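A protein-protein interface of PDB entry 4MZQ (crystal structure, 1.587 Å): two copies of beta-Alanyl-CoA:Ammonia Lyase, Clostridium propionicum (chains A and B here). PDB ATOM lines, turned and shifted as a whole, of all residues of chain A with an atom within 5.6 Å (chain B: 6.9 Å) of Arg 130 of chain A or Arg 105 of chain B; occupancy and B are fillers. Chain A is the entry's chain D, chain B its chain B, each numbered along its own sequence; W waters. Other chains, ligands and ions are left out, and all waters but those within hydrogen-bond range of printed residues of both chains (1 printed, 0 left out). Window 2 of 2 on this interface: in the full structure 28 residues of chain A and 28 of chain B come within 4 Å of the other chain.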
ATOM      1  N   ASP A  45     -36.881 -15.538 -21.104  1.00  0.00           N
ATOM      2  CA  ASP A  45     -36.116 -16.634 -21.700  1.00  0.00           C
ATOM      3  C   ASP A  45     -34.673 -16.772 -21.194  1.00  0.00           C
ATOM      4  O   ASP A  45     -33.859 -17.483 -21.799  1.00  0.00           O
ATOM      5  CB  ASP A  45     -36.123 -16.506 -23.234  1.00  0.00           C
ATOM      6  CG  ASP A  45     -37.116 -17.471 -23.899  1.00  0.00           C
ATOM      7  OD1 ASP A  45     -37.901 -17.030 -24.761  1.00  0.00           O
ATOM      8  OD2 ASP A  45     -37.114 -18.674 -23.558  1.00  0.00           O
ATOM      9  N   GLY A  46     -34.345 -16.098 -20.096  1.00  0.00           N
ATOM     10  CA  GLY A  46     -33.087 -16.364 -19.409  1.00  0.00           C
ATOM     11  C   GLY A  46     -31.800 -15.920 -20.094  1.00  0.00           C
ATOM     12  O   GLY A  46     -30.753 -16.548 -19.910  1.00  0.00           O
ATOM     13  N   ASP A  47     -31.878 -14.838 -20.864  1.00  0.00           N
ATOM     14  CA  ASP A  47     -30.725 -14.299 -21.571  1.00  0.00           C
ATOM     15  C   ASP A  47     -30.795 -12.785 -21.542  1.00  0.00           C
ATOM     16  O   ASP A  47     -31.896 -12.229 -21.610  1.00  0.00           O
ATOM     17  CB  ASP A  47     -30.698 -14.812 -23.010  1.00  0.00           C
ATOM     18  CG  ASP A  47     -29.358 -14.604 -23.680  1.00  0.00           C
ATOM     19  OD1 ASP A  47     -29.149 -13.537 -24.291  1.00  0.00           O
ATOM     20  OD2 ASP A  47     -28.501 -15.508 -23.582  1.00  0.00           O
ATOM     21  N   ILE A  48     -29.643 -12.122 -21.430  1.00  0.00           N
ATOM     22  CA  ILE A  48     -29.647 -10.656 -21.396  1.00  0.00           C
ATOM     23  C   ILE A  48     -30.027 -10.058 -22.749  1.00  0.00           C
ATOM     24  O   ILE A  48     -30.417  -8.893 -22.809  1.00  0.00           O
ATOM     25  CB  ILE A  48     -28.290 -10.052 -20.932  1.00  0.00           C
ATOM     26  CG1 ILE A  48     -27.115 -10.511 -21.809  1.00  0.00           C
ATOM     27  CG2 ILE A  48     -28.054 -10.363 -19.452  1.00  0.00           C
ATOM     28  CD1 ILE A  48     -25.773  -9.821 -21.485  1.00  0.00           C
ATOM     29  N   ASN A 128     -30.201 -19.845 -27.363  1.00  0.00           N
ATOM     30  CA  ASN A 128     -30.011 -19.165 -26.087  1.00  0.00           C
ATOM     31  C   ASN A 128     -31.321 -19.008 -25.315  1.00  0.00           C
ATOM     32  O   ASN A 128     -31.330 -18.488 -24.194  1.00  0.00           O
ATOM     33  CB  ASN A 128     -29.373 -17.781 -26.291  1.00  0.00           C
ATOM     34  CG  ASN A 128     -27.916 -17.861 -26.717  1.00  0.00           C
ATOM     35  OD1 ASN A 128     -27.187 -18.773 -26.325  1.00  0.00           O
ATOM     36  ND2 ASN A 128     -27.486 -16.904 -27.527  1.00  0.00           N
ATOM     37  N   GLN A 129     -32.428 -19.435 -25.914  1.00  0.00           N
ATOM     38  CA  GLN A 129     -33.717 -19.352 -25.243  1.00  0.00           C
ATOM     39  C   GLN A 129     -33.840 -20.491 -24.233  1.00  0.00           C
ATOM     40  O   GLN A 129     -33.785 -21.665 -24.597  1.00  0.00           O
ATOM     41  CB  GLN A 129     -34.867 -19.383 -26.255  1.00  0.00           C
ATOM     42  CG  GLN A 129     -34.831 -18.217 -27.242  1.00  0.00           C
ATOM     43  CD  GLN A 129     -35.965 -18.255 -28.246  1.00  0.00           C
ATOM     44  OE1 GLN A 129     -36.903 -19.053 -28.122  1.00  0.00           O
ATOM     45  NE2 GLN A 129     -35.889 -17.385 -29.251  1.00  0.00           N
ATOM     46  N   ARG A 130     -34.010 -20.132 -22.965  1.00  0.00           N
ATOM     47  CA  ARG A 130     -33.961 -21.117 -21.890  1.00  0.00           C
ATOM     48  C   ARG A 130     -35.288 -21.223 -21.153  1.00  0.00           C
ATOM     49  O   ARG A 130     -35.389 -21.920 -20.141  1.00  0.00           O
ATOM     50  CB  ARG A 130     -32.843 -20.762 -20.907  1.00  0.00           C
ATOM     51  CG  ARG A 130     -31.501 -20.498 -21.578  1.00  0.00           C
ATOM     52  CD  ARG A 130     -30.372 -20.476 -20.569  1.00  0.00           C
ATOM     53  NE  ARG A 130     -30.559 -19.418 -19.583  1.00  0.00           N
ATOM     54  CZ  ARG A 130     -30.732 -19.620 -18.278  1.00  0.00           C
ATOM     55  NH1 ARG A 130     -30.723 -20.846 -17.765  1.00  0.00           N
ATOM     56  NH2 ARG A 130     -30.894 -18.579 -17.473  1.00  0.00           N
ATOM     57  N   GLY A 131     -36.302 -20.528 -21.657  1.00  0.00           N
ATOM     58  CA  GLY A 131     -37.616 -20.528 -21.038  1.00  0.00           C
ATOM     59  C   GLY A 131     -37.738 -19.520 -19.911  1.00  0.00           C
ATOM     60  O   GLY A 131     -36.736 -18.922 -19.499  1.00  0.00           O
ATOM     61  N   PRO A 132     -38.969 -19.323 -19.403  1.00  0.00           N
ATOM     62  CA  PRO A 132     -39.250 -18.313 -18.376  1.00  0.00           C
ATOM     63  C   PRO A 132     -38.418 -18.497 -17.110  1.00  0.00           C
ATOM     64  O   PRO A 132     -38.190 -19.623 -16.668  1.00  0.00           O
ATOM     65  CB  PRO A 132     -40.741 -18.514 -18.080  1.00  0.00           C
ATOM     66  CG  PRO A 132     -41.280 -19.134 -19.326  1.00  0.00           C
ATOM     67  CD  PRO A 132     -40.192 -20.023 -19.836  1.00  0.00           C
ATOM     68  N   GLN A 133     -37.955 -17.387 -16.546  1.00  0.00           N
ATOM     69  CA  GLN A 133     -37.112 -17.430 -15.356  1.00  0.00           C
ATOM     70  C   GLN A 133     -37.792 -16.778 -14.161  1.00  0.00           C
ATOM     71  O   GLN A 133     -37.285 -16.826 -13.041  1.00  0.00           O
ATOM     72  CB  GLN A 133     -35.777 -16.738 -15.637  1.00  0.00           C
ATOM     73  CG  GLN A 133     -35.001 -17.390 -16.759  1.00  0.00           C
ATOM     74  CD  GLN A 133     -34.553 -18.796 -16.406  1.00  0.00           C
ATOM     75  OE1 GLN A 133     -34.043 -19.035 -15.313  1.00  0.00           O
ATOM     76  NE2 GLN A 133     -34.762 -19.741 -17.322  1.00  0.00           N
ATOM     77  N   LYS B  94     -29.953 -11.657 -11.823  1.00  0.00           N
ATOM     78  CA  LYS B  94     -28.492 -11.779 -11.858  1.00  0.00           C
ATOM     79  C   LYS B  94     -28.037 -12.571 -13.072  1.00  0.00           C
ATOM     80  O   LYS B  94     -28.819 -13.327 -13.651  1.00  0.00           O
ATOM     81  CB  LYS B  94     -27.988 -12.471 -10.588  1.00  0.00           C
ATOM     82  CG  LYS B  94     -28.481 -13.914 -10.464  1.00  0.00           C
ATOM     83  CD  LYS B  94     -27.893 -14.612  -9.247  1.00  0.00           C
ATOM     84  CE  LYS B  94     -28.234 -16.093  -9.279  1.00  0.00           C
ATOM     85  NZ  LYS B  94     -27.624 -16.837  -8.145  1.00  0.00           N
ATOM     86  N   MET B  95     -26.768 -12.422 -13.447  1.00  0.00           N
ATOM     87  CA  MET B  95     -26.157 -13.332 -14.404  1.00  0.00           C
ATOM     88  C   MET B  95     -26.018 -14.700 -13.748  1.00  0.00           C
ATOM     89  O   MET B  95     -25.815 -14.790 -12.540  1.00  0.00           O
ATOM     90  CB  MET B  95     -24.772 -12.841 -14.852  1.00  0.00           C
ATOM     91  CG  MET B  95     -24.721 -11.415 -15.334  1.00  0.00           C
ATOM     92  SD  MET B  95     -25.693 -11.142 -16.820  1.00  0.00           S
ATOM     93  CE  MET B  95     -24.897 -12.241 -18.005  1.00  0.00           C
ATOM     94  N   VAL B  96     -26.106 -15.756 -14.543  1.00  0.00           N
ATOM     95  CA  VAL B  96     -25.957 -17.114 -14.035  1.00  0.00           C
ATOM     96  C   VAL B  96     -24.509 -17.412 -13.648  1.00  0.00           C
ATOM     97  O   VAL B  96     -24.251 -18.141 -12.687  1.00  0.00           O
ATOM     98  CB  VAL B  96     -26.470 -18.126 -15.077  1.00  0.00           C
ATOM     99  CG1 VAL B  96     -26.069 -19.568 -14.724  1.00  0.00           C
ATOM    100  CG2 VAL B  96     -27.993 -17.986 -15.209  1.00  0.00           C
ATOM    101  N   ASP B  97     -23.560 -16.831 -14.375  1.00  0.00           N
ATOM    102  CA  ASP B  97     -22.149 -17.085 -14.083  1.00  0.00           C
ATOM    103  C   ASP B  97     -21.234 -15.872 -14.357  1.00  0.00           C
ATOM    104  O   ASP B  97     -20.710 -15.716 -15.464  1.00  0.00           O
ATOM    105  CB  ASP B  97     -21.686 -18.303 -14.885  1.00  0.00           C
ATOM    106  CG  ASP B  97     -20.251 -18.705 -14.576  1.00  0.00           C
ATOM    107  OD1 ASP B  97     -19.687 -18.218 -13.582  1.00  0.00           O
ATOM    108  OD2 ASP B  97     -19.691 -19.510 -15.341  1.00  0.00           O
ATOM    109  N   ASN B 100     -17.624 -15.953 -16.032  1.00  0.00           N
ATOM    110  CA  ASN B 100     -17.444 -16.153 -17.463  1.00  0.00           C
ATOM    111  C   ASN B 100     -17.989 -14.960 -18.245  1.00  0.00           C
ATOM    112  O   ASN B 100     -19.191 -14.863 -18.477  1.00  0.00           O
ATOM    113  CB  ASN B 100     -18.120 -17.452 -17.905  1.00  0.00           C
ATOM    114  CG  ASN B 100     -17.903 -17.760 -19.375  1.00  0.00           C
ATOM    115  OD1 ASN B 100     -16.997 -17.221 -20.015  1.00  0.00           O
ATOM    116  ND2 ASN B 100     -18.740 -18.640 -19.917  1.00  0.00           N
ATOM    117  N   GLN B 102     -18.224 -13.974 -21.240  1.00  0.00           N
ATOM    118  CA  GLN B 102     -18.957 -14.161 -22.490  1.00  0.00           C
ATOM    119  C   GLN B 102     -20.335 -14.800 -22.300  1.00  0.00           C
ATOM    120  O   GLN B 102     -21.160 -14.791 -23.213  1.00  0.00           O
ATOM    121  CB  GLN B 102     -18.132 -15.013 -23.458  1.00  0.00           C
ATOM    122  CG  GLN B 102     -17.077 -14.233 -24.233  1.00  0.00           C
ATOM    123  CD  GLN B 102     -16.141 -13.465 -23.327  1.00  0.00           C
ATOM    124  OE1 GLN B 102     -15.413 -14.055 -22.530  1.00  0.00           O
ATOM    125  NE2 GLN B 102     -16.163 -12.138 -23.435  1.00  0.00           N
ATOM    126  N   ASP B 103     -20.576 -15.354 -21.121  1.00  0.00           N
ATOM    127  CA  ASP B 103     -21.841 -16.009 -20.811  1.00  0.00           C
ATOM    128  C   ASP B 103     -22.940 -14.952 -20.781  1.00  0.00           C
ATOM    129  O   ASP B 103     -22.771 -13.908 -20.152  1.00  0.00           O
ATOM    130  CB  ASP B 103     -21.730 -16.739 -19.470  1.00  0.00           C
ATOM    131  CG  ASP B 103     -22.823 -17.777 -19.260  1.00  0.00           C
ATOM    132  OD1 ASP B 103     -23.911 -17.641 -19.844  1.00  0.00           O
ATOM    133  OD2 ASP B 103     -22.583 -18.730 -18.482  1.00  0.00           O
ATOM    134  N   THR B 104     -24.055 -15.205 -21.463  1.00  0.00           N
ATOM    135  CA  THR B 104     -25.152 -14.240 -21.481  1.00  0.00           C
ATOM    136  C   THR B 104     -26.371 -14.743 -20.715  1.00  0.00           C
ATOM    137  O   THR B 104     -27.405 -14.072 -20.696  1.00  0.00           O
ATOM    138  CB  THR B 104     -25.584 -13.889 -22.918  1.00  0.00           C
ATOM    139  OG1 THR B 104     -25.839 -15.093 -23.652  1.00  0.00           O
ATOM    140  CG2 THR B 104     -24.484 -13.116 -23.622  1.00  0.00           C
ATOM    141  N   ARG B 105     -26.247 -15.904 -20.076  1.00  0.00           N
ATOM    142  CA  ARG B 105     -27.348 -16.446 -19.270  1.00  0.00           C
ATOM    143  C   ARG B 105     -27.621 -15.594 -18.028  1.00  0.00           C
ATOM    144  O   ARG B 105     -26.704 -15.091 -17.380  1.00  0.00           O
ATOM    145  CB  ARG B 105     -27.049 -17.892 -18.861  1.00  0.00           C
ATOM    146  CG  ARG B 105     -26.934 -18.843 -20.050  1.00  0.00           C
ATOM    147  CD  ARG B 105     -26.495 -20.238 -19.607  1.00  0.00           C
ATOM    148  NE  ARG B 105     -25.164 -20.229 -19.008  1.00  0.00           N
ATOM    149  CZ  ARG B 105     -24.673 -21.213 -18.263  1.00  0.00           C
ATOM    150  NH1 ARG B 105     -25.404 -22.294 -18.019  1.00  0.00           N
ATOM    151  NH2 ARG B 105     -23.447 -21.119 -17.770  1.00  0.00           N
ATOM    152  N   ALA B 106     -28.900 -15.405 -17.722  1.00  0.00           N
ATOM    153  CA  ALA B 106     -29.287 -14.671 -16.534  1.00  0.00           C
ATOM    154  C   ALA B 106     -30.622 -15.191 -16.044  1.00  0.00           C
ATOM    155  O   ALA B 106     -31.351 -15.859 -16.778  1.00  0.00           O
ATOM    156  CB  ALA B 106     -29.351 -13.172 -16.822  1.00  0.00           C
ATOM    157  N   THR B 107     -30.936 -14.909 -14.793  1.00  0.00           N
ATOM    158  CA  THR B 107     -32.152 -15.453 -14.211  1.00  0.00           C
ATOM    159  C   THR B 107     -32.673 -14.512 -13.130  1.00  0.00           C
ATOM    160  O   THR B 107     -31.980 -13.588 -12.717  1.00  0.00           O
ATOM    161  CB  THR B 107     -31.901 -16.869 -13.637  1.00  0.00           C
ATOM    162  OG1 THR B 107     -33.154 -17.520 -13.367  1.00  0.00           O
ATOM    163  CG2 THR B 107     -31.058 -16.810 -12.385  1.00  0.00           C
ATOM    164  N   ALA B 108     -33.901 -14.744 -12.674  1.00  0.00           N
ATOM    165  CA  ALA B 108     -34.430 -13.956 -11.577  1.00  0.00           C
ATOM    166  C   ALA B 108     -33.991 -14.551 -10.253  1.00  0.00           C
ATOM    167  O   ALA B 108     -33.671 -15.739 -10.171  1.00  0.00           O
ATOM    168  CB  ALA B 108     -35.948 -13.886 -11.641  1.00  0.00           C
HETATM  169  O   HOH W   1     -24.951 -15.348 -26.189  1.00  0.00           O
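The side-chain carboxylate (OD2) of Asp 47 of chain A sits at hydrogen-bond distance from the side-chain hydroxyl (OG1) of Thr 104 of chain B (2.7 Å).
The backbone NH (N) of Ile 48 of chain A lies within hydrogen-bond range of the backbone carbonyl oxygen (O) of Thr 104 of chain B (3.1 Å).
O of Gly 46 of chain A sits at hydrogen-bond distance from N of Ala 106 of chain B, 3.1 Å away.
The backbone carbonyl oxygen of Ala 106 of chain B sits at hydrogen-bond distance from the guanidinium group of Arg 130 of chain A (2.8 Å).
The side-chain amide oxygen (OE1) of Gln 133 of chain A is in hydrogen-bond range of the side-chain hydroxyl (OG1) of Thr 107 of chain B (2.6 Å).
Water W1 bridges OG1 of Thr 104 of chain B and ND2 of Asn 128 of chain A.
Arg 105 of chain B touches Gly 46 of chain A (CA to O, 3.5 Å).
Met 95 of chain B touches Ile 48 of chain A.
NH2 of Arg 130 of chain A touches CG2 of Val 96 of chain B (3.7 Å).
Arg 105 of chain B touches Arg 130 of chain A (CG to NE, 3.7 Å).
CG of Gln 133 of chain A touches O of Ala 106 of chain B (3.96 Å).
O of Gln 133 of chain A touches CB of Ala 108 of chain B (3.5 Å).
Of the 12 printed residues of chain B, 7 touch a printed residue of chain A.
Hydrophobic or aromatic side chains of chain B that line the printed part of chain A: Met 95, Val 96 and Ala 108.
Hydrophobic or aromatic side chains of chain A within 4 Å of the printed part of chain B: Ile 48.
Among the printed residues, 11 pairs touch across the chains.
Among the printed residues, no Asp or Glu carboxylate lies within 4 Å of a Lys or Arg side-chain nitrogen of the other chain.
The backbone NH (N) of Thr 107 of chain B lies within hydrogen-bond range of the backbone carbonyl oxygen (O) of Lys 94 of chain B (2.9 Å).
N of Val 96 of chain B is in hydrogen-bond range of O of Arg 105 of chain B.
The side-chain carboxylate of Asp 103 of chain B lies within salt-bridge range of the guanidinium group of Arg 105 of chain B (2.6 Å).
O of Asp 45 of chain A is in hydrogen-bond range of N of Arg 130 of chain A (2.9 Å).
The backbone carbonyl oxygen (O) of Gly 46 of chain A lies within hydrogen-bond range of the guanidinium group (NE) of Arg 130 of chain A (2.9 Å).
The backbone carbonyl oxygen (O) of Gly 131 of chain A lies within hydrogen-bond range of the side-chain amide nitrogen (NE2) of Gln 133 of chain A.
No position is printed for both chains.
Of the 11 pairs that touch across the chains among the printed residues, none has its exchanged pair printed and touching as well.
Arg 105 of chain B touches just these residues of chain A: Gly 46 and Arg 130.
Of the printed residues of chain A, Met 95 of chain B touches Ile 48.
Of the printed residues of chain A, Val 96 of chain B touches Arg 130 (3.7 Å).
Of the printed residues of chain B, Ile 48 of chain A touches Met 95 and Thr 104.
The nearest residue of chain B that does not touch Arg 130 of chain A is Thr 107 of chain B (4.3 Å).
The nearest printed residue of chain B that does not touch Gln 133 of chain A is Val 96 of chain B (6.1 Å).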
